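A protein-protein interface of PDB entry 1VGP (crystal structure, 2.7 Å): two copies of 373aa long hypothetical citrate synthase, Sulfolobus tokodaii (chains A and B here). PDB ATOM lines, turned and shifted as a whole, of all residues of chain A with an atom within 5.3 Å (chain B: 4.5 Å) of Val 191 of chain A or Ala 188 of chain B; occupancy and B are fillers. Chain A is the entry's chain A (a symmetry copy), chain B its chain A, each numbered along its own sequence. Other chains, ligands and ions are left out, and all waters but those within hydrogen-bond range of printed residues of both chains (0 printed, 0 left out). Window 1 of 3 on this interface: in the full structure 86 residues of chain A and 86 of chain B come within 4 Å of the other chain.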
ATOM      1  N   PHE A 187      -7.710   2.075 -24.471  1.00  0.00           N
ATOM      2  CA  PHE A 187      -7.336   0.698 -24.205  1.00  0.00           C
ATOM      3  C   PHE A 187      -8.581  -0.209 -24.130  1.00  0.00           C
ATOM      4  O   PHE A 187      -8.563  -1.352 -24.600  1.00  0.00           O
ATOM      5  CB  PHE A 187      -6.544   0.628 -22.898  1.00  0.00           C
ATOM      6  CG  PHE A 187      -5.992  -0.729 -22.594  1.00  0.00           C
ATOM      7  CD1 PHE A 187      -6.308  -1.368 -21.390  1.00  0.00           C
ATOM      8  CD2 PHE A 187      -5.138  -1.368 -23.491  1.00  0.00           C
ATOM      9  CE1 PHE A 187      -5.775  -2.629 -21.083  1.00  0.00           C
ATOM     10  CE2 PHE A 187      -4.601  -2.626 -23.199  1.00  0.00           C
ATOM     11  CZ  PHE A 187      -4.921  -3.259 -21.989  1.00  0.00           C
ATOM     12  N   ALA A 188      -9.662   0.304 -23.549  1.00  0.00           N
ATOM     13  CA  ALA A 188     -10.914  -0.446 -23.504  1.00  0.00           C
ATOM     14  C   ALA A 188     -11.342  -0.786 -24.930  1.00  0.00           C
ATOM     15  O   ALA A 188     -11.774  -1.909 -25.201  1.00  0.00           O
ATOM     16  CB  ALA A 188     -12.002   0.374 -22.798  1.00  0.00           C
ATOM     17  N   SER A 189     -11.210   0.192 -25.827  1.00  0.00           N
ATOM     18  CA  SER A 189     -11.424   0.011 -27.264  1.00  0.00           C
ATOM     19  C   SER A 189     -10.620  -1.161 -27.805  1.00  0.00           C
ATOM     20  O   SER A 189     -11.151  -2.033 -28.490  1.00  0.00           O
ATOM     21  CB  SER A 189     -10.976   1.265 -28.019  1.00  0.00           C
ATOM     22  OG  SER A 189     -12.077   2.098 -28.272  1.00  0.00           O
ATOM     23  N   LEU A 190      -9.325  -1.138 -27.502  1.00  0.00           N
ATOM     24  CA  LEU A 190      -8.379  -2.092 -28.042  1.00  0.00           C
ATOM     25  C   LEU A 190      -8.677  -3.506 -27.520  1.00  0.00           C
ATOM     26  O   LEU A 190      -8.540  -4.492 -28.254  1.00  0.00           O
ATOM     27  CB  LEU A 190      -6.954  -1.673 -27.661  1.00  0.00           C
ATOM     28  CG  LEU A 190      -6.071  -0.962 -28.692  1.00  0.00           C
ATOM     29  CD1 LEU A 190      -6.888  -0.436 -29.870  1.00  0.00           C
ATOM     30  CD2 LEU A 190      -5.323   0.175 -27.989  1.00  0.00           C
ATOM     31  N   VAL A 191      -9.087  -3.604 -26.262  1.00  0.00           N
ATOM     32  CA  VAL A 191      -9.420  -4.898 -25.707  1.00  0.00           C
ATOM     33  C   VAL A 191     -10.558  -5.532 -26.498  1.00  0.00           C
ATOM     34  O   VAL A 191     -10.493  -6.706 -26.881  1.00  0.00           O
ATOM     35  CB  VAL A 191      -9.841  -4.793 -24.229  1.00  0.00           C
ATOM     36  CG1 VAL A 191     -10.171  -6.190 -23.691  1.00  0.00           C
ATOM     37  CG2 VAL A 191      -8.725  -4.125 -23.406  1.00  0.00           C
ATOM     38  N   VAL A 192     -11.607  -4.760 -26.748  1.00  0.00           N
ATOM     39  CA  VAL A 192     -12.726  -5.271 -27.521  1.00  0.00           C
ATOM     40  C   VAL A 192     -12.282  -5.549 -28.964  1.00  0.00           C
ATOM     41  O   VAL A 192     -12.583  -6.606 -29.526  1.00  0.00           O
ATOM     42  CB  VAL A 192     -13.900  -4.275 -27.494  1.00  0.00           C
ATOM     43  CG1 VAL A 192     -14.973  -4.693 -28.483  1.00  0.00           C
ATOM     44  CG2 VAL A 192     -14.479  -4.217 -26.082  1.00  0.00           C
ATOM     45  N   ALA A 193     -11.549  -4.611 -29.553  1.00  0.00           N
ATOM     46  CA  ALA A 193     -11.134  -4.766 -30.933  1.00  0.00           C
ATOM     47  C   ALA A 193     -10.262  -6.006 -31.120  1.00  0.00           C
ATOM     48  O   ALA A 193     -10.293  -6.641 -32.174  1.00  0.00           O
ATOM     49  CB  ALA A 193     -10.384  -3.516 -31.415  1.00  0.00           C
ATOM     50  N   SER A 194      -9.491  -6.364 -30.098  1.00  0.00           N
ATOM     51  CA  SER A 194      -8.503  -7.426 -30.254  1.00  0.00           C
ATOM     52  C   SER A 194      -9.163  -8.793 -30.283  1.00  0.00           C
ATOM     53  O   SER A 194      -8.502  -9.803 -30.517  1.00  0.00           O
ATOM     54  CB  SER A 194      -7.478  -7.386 -29.122  1.00  0.00           C
ATOM     55  OG  SER A 194      -8.035  -7.906 -27.932  1.00  0.00           O
ATOM     56  N   THR A 195     -10.470  -8.830 -30.041  1.00  0.00           N
ATOM     57  CA  THR A 195     -11.235 -10.065 -30.206  1.00  0.00           C
ATOM     58  C   THR A 195     -11.924 -10.056 -31.564  1.00  0.00           C
ATOM     59  O   THR A 195     -12.657 -10.983 -31.907  1.00  0.00           O
ATOM     60  CB  THR A 195     -12.311 -10.217 -29.119  1.00  0.00           C
ATOM     61  OG1 THR A 195     -13.396  -9.330 -29.404  1.00  0.00           O
ATOM     62  CG2 THR A 195     -11.741  -9.886 -27.760  1.00  0.00           C
ATOM     63  N   ILE A 353      -6.258  -9.598 -26.314  1.00  0.00           N
ATOM     64  CA  ILE A 353      -5.697  -9.184 -25.044  1.00  0.00           C
ATOM     65  C   ILE A 353      -6.359  -9.979 -23.940  1.00  0.00           C
ATOM     66  O   ILE A 353      -7.482  -9.687 -23.544  1.00  0.00           O
ATOM     67  CB  ILE A 353      -5.923  -7.672 -24.790  1.00  0.00           C
ATOM     68  CG1 ILE A 353      -5.152  -6.851 -25.813  1.00  0.00           C
ATOM     69  CG2 ILE A 353      -5.456  -7.314 -23.393  1.00  0.00           C
ATOM     70  CD1 ILE A 353      -5.728  -5.460 -26.050  1.00  0.00           C
ATOM     71  N   ALA B 184     -10.504 -11.644 -22.322  1.00  0.00           N
ATOM     72  CA  ALA B 184     -10.767 -10.364 -22.965  1.00  0.00           C
ATOM     73  C   ALA B 184     -12.030  -9.699 -22.432  1.00  0.00           C
ATOM     74  O   ALA B 184     -12.031  -8.498 -22.167  1.00  0.00           O
ATOM     75  CB  ALA B 184     -10.864 -10.554 -24.462  1.00  0.00           C
ATOM     76  N   SER B 185     -13.106 -10.466 -22.271  1.00  0.00           N
ATOM     77  CA  SER B 185     -14.392  -9.866 -21.920  1.00  0.00           C
ATOM     78  C   SER B 185     -14.477  -9.477 -20.440  1.00  0.00           C
ATOM     79  O   SER B 185     -14.965  -8.403 -20.101  1.00  0.00           O
ATOM     80  CB  SER B 185     -15.542 -10.807 -22.290  1.00  0.00           C
ATOM     81  OG  SER B 185     -15.383 -12.078 -21.699  1.00  0.00           O
ATOM     82  N   THR B 186     -14.001 -10.347 -19.560  1.00  0.00           N
ATOM     83  CA  THR B 186     -13.953 -10.019 -18.143  1.00  0.00           C
ATOM     84  C   THR B 186     -13.027  -8.834 -17.937  1.00  0.00           C
ATOM     85  O   THR B 186     -13.271  -7.981 -17.084  1.00  0.00           O
ATOM     86  CB  THR B 186     -13.435 -11.203 -17.325  1.00  0.00           C
ATOM     87  OG1 THR B 186     -14.295 -12.325 -17.539  1.00  0.00           O
ATOM     88  CG2 THR B 186     -13.400 -10.870 -15.843  1.00  0.00           C
ATOM     89  N   PHE B 187     -11.963  -8.787 -18.725  1.00  0.00           N
ATOM     90  CA  PHE B 187     -10.974  -7.732 -18.592  1.00  0.00           C
ATOM     91  C   PHE B 187     -11.496  -6.407 -19.184  1.00  0.00           C
ATOM     92  O   PHE B 187     -11.249  -5.327 -18.637  1.00  0.00           O
ATOM     93  CB  PHE B 187      -9.679  -8.156 -19.288  1.00  0.00           C
ATOM     94  CG  PHE B 187      -8.546  -7.198 -19.099  1.00  0.00           C
ATOM     95  CD1 PHE B 187      -7.901  -6.636 -20.207  1.00  0.00           C
ATOM     96  CD2 PHE B 187      -8.100  -6.866 -17.821  1.00  0.00           C
ATOM     97  CE1 PHE B 187      -6.821  -5.757 -20.041  1.00  0.00           C
ATOM     98  CE2 PHE B 187      -7.024  -5.989 -17.641  1.00  0.00           C
ATOM     99  CZ  PHE B 187      -6.381  -5.433 -18.756  1.00  0.00           C
ATOM    100  N   ALA B 188     -12.223  -6.492 -20.294  1.00  0.00           N
ATOM    101  CA  ALA B 188     -12.830  -5.302 -20.884  1.00  0.00           C
ATOM    102  C   ALA B 188     -13.743  -4.645 -19.850  1.00  0.00           C
ATOM    103  O   ALA B 188     -13.741  -3.421 -19.705  1.00  0.00           O
ATOM    104  CB  ALA B 188     -13.626  -5.677 -22.141  1.00  0.00           C
ATOM    105  N   SER B 189     -14.508  -5.474 -19.139  1.00  0.00           N
ATOM    106  CA  SER B 189     -15.331  -5.046 -18.005  1.00  0.00           C
ATOM    107  C   SER B 189     -14.519  -4.257 -16.992  1.00  0.00           C
ATOM    108  O   SER B 189     -14.908  -3.168 -16.576  1.00  0.00           O
ATOM    109  CB  SER B 189     -15.901  -6.272 -17.286  1.00  0.00           C
ATOM    110  OG  SER B 189     -17.205  -6.536 -17.737  1.00  0.00           O
ATOM    111  N   LEU B 190     -13.399  -4.852 -16.587  1.00  0.00           N
ATOM    112  CA  LEU B 190     -12.569  -4.318 -15.528  1.00  0.00           C
ATOM    113  C   LEU B 190     -11.940  -2.982 -15.952  1.00  0.00           C
ATOM    114  O   LEU B 190     -11.805  -2.060 -15.139  1.00  0.00           O
ATOM    115  CB  LEU B 190     -11.477  -5.332 -15.171  1.00  0.00           C
ATOM    116  CG  LEU B 190     -11.636  -6.214 -13.928  1.00  0.00           C
ATOM    117  CD1 LEU B 190     -13.072  -6.208 -13.410  1.00  0.00           C
ATOM    118  CD2 LEU B 190     -11.185  -7.635 -14.280  1.00  0.00           C
ATOM    119  N   VAL B 191     -11.562  -2.876 -17.220  1.00  0.00           N
ATOM    120  CA  VAL B 191     -10.992  -1.639 -17.706  1.00  0.00           C
ATOM    121  C   VAL B 191     -11.990  -0.499 -17.539  1.00  0.00           C
ATOM    122  O   VAL B 191     -11.651   0.579 -17.038  1.00  0.00           O
ATOM    123  CB  VAL B 191     -10.593  -1.738 -19.189  1.00  0.00           C
ATOM    124  CG1 VAL B 191      -9.987  -0.407 -19.647  1.00  0.00           C
ATOM    125  CG2 VAL B 191      -9.610  -2.903 -19.398  1.00  0.00           C
ATOM    126  N   VAL B 192     -13.227  -0.731 -17.959  1.00  0.00           N
ATOM    127  CA  VAL B 192     -14.253   0.288 -17.815  1.00  0.00           C
ATOM    128  C   VAL B 192     -14.544   0.529 -16.327  1.00  0.00           C
ATOM    129  O   VAL B 192     -14.621   1.677 -15.875  1.00  0.00           O
ATOM    130  CB  VAL B 192     -15.534  -0.127 -18.560  1.00  0.00           C
ATOM    131  CG1 VAL B 192     -16.675   0.815 -18.219  1.00  0.00           C
ATOM    132  CG2 VAL B 192     -15.269  -0.111 -20.063  1.00  0.00           C
ATOM    133  N   ALA B 205     -19.305  -3.270 -22.069  1.00  0.00           N
ATOM    134  CA  ALA B 205     -17.959  -3.587 -22.545  1.00  0.00           C
ATOM    135  C   ALA B 205     -17.715  -5.099 -22.491  1.00  0.00           C
ATOM    136  O   ALA B 205     -17.130  -5.666 -23.409  1.00  0.00           O
ATOM    137  CB  ALA B 205     -16.928  -2.864 -21.692  1.00  0.00           C
ATOM    138  N   ALA B 209     -16.977  -7.406 -25.873  1.00  0.00           N
ATOM    139  CA  ALA B 209     -15.790  -8.225 -26.076  1.00  0.00           C
ATOM    140  C   ALA B 209     -16.185  -9.685 -26.266  1.00  0.00           C
ATOM    141  O   ALA B 209     -15.641 -10.374 -27.130  1.00  0.00           O
ATOM    142  CB  ALA B 209     -14.834  -8.083 -24.891  1.00  0.00           C
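The backbone carbonyl oxygen (O) of Ala 209 of chain B lies within hydrogen-bond range of the side-chain hydroxyl (OG1) of Thr 195 of chain A, at 3.4 Å.
The backbone carbonyl oxygen of Val 191 of chain A lies within hydrogen-bond range of the side-chain hydroxyl of Ser 194 of chain A, 2.9 Å away. The backbone carbonyl oxygen of Val 192 of chain A sits at hydrogen-bond distance from the side-chain hydroxyl of Thr 195 of chain A. The side-chain hydroxyl of Ser 194 of chain A lies within hydrogen-bond range of the backbone NH of Ile 353 of chain A (2.9 Å).
CE1 of Phe 187 of chain B touches CE1 of Phe 187 of chain A (3.5 Å). CG1 of Val 191 of chain B touches CB of Ala 188 of chain A, at 3.8 Å. Val 191 of chain A touches Ala 184 of chain B. CG1 of Val 191 of chain A touches CB of Ala 188 of chain B, 3.8 Å away. Thr 195 of chain A touches Ala 184 of chain B. Ala 184 of chain B touches Ile 353 of chain A. Ile 353 of chain A touches Phe 187 of chain B.
Printed residues of chain B within 4 Å of Phe 187 of chain A: Phe 187. Val 191 of chain A touches just these residues of chain B: Ala 184 (3.3 Å) and Ala 188 (3.8 Å). Printed residues of chain B within 4 Å of Thr 195 of chain A: Ala 184 (3.5 Å) and Ala 209 (3.4 Å). Of the printed residues of chain A, Ala 184 of chain B touches Val 191, Thr 195 and Ile 353. Printed residues of chain A within 4 Å of Ala 209 of chain B: Thr 195. The nearest residue of chain B that does not touch Val 191 of chain A is Phe 187 of chain B (4.1 Å). The nearest residue of chain A that does not touch Ala 188 of chain B is Val 192 of chain A (4.3 Å). The nearest printed residue of chain B that does not touch Ala 188 of chain A is Val 192 of chain B (4.3 Å).
Hydrophobic or aromatic side chains of chain A within 4 Å of the printed part of chain B: Phe 187, Ala 188, Val 191 and Ile 353. Of the 11 printed residues of chain B, 5 touch a printed residue of chain A. Printed residues of chain B that touch a printed residue of chain A: Ala 184, Phe 187, Ala 188, Val 191 and Ala 209. Hydrophobic or aromatic side chains of chain B that line the printed part of chain A: Ala 184, Phe 187, Ala 188 and Val 191. Among the printed residues, no Asp or Glu carboxylate lies within 4 Å of a Lys or Arg side-chain nitrogen of the other chain.
Phe 187 of chain B touches its own counterpart, Phe 187 of chain A. Ala 188 of chain A touches Val 191 of chain B, and with the chains exchanged Val 191 of chain A touches Ala 188 of chain B.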
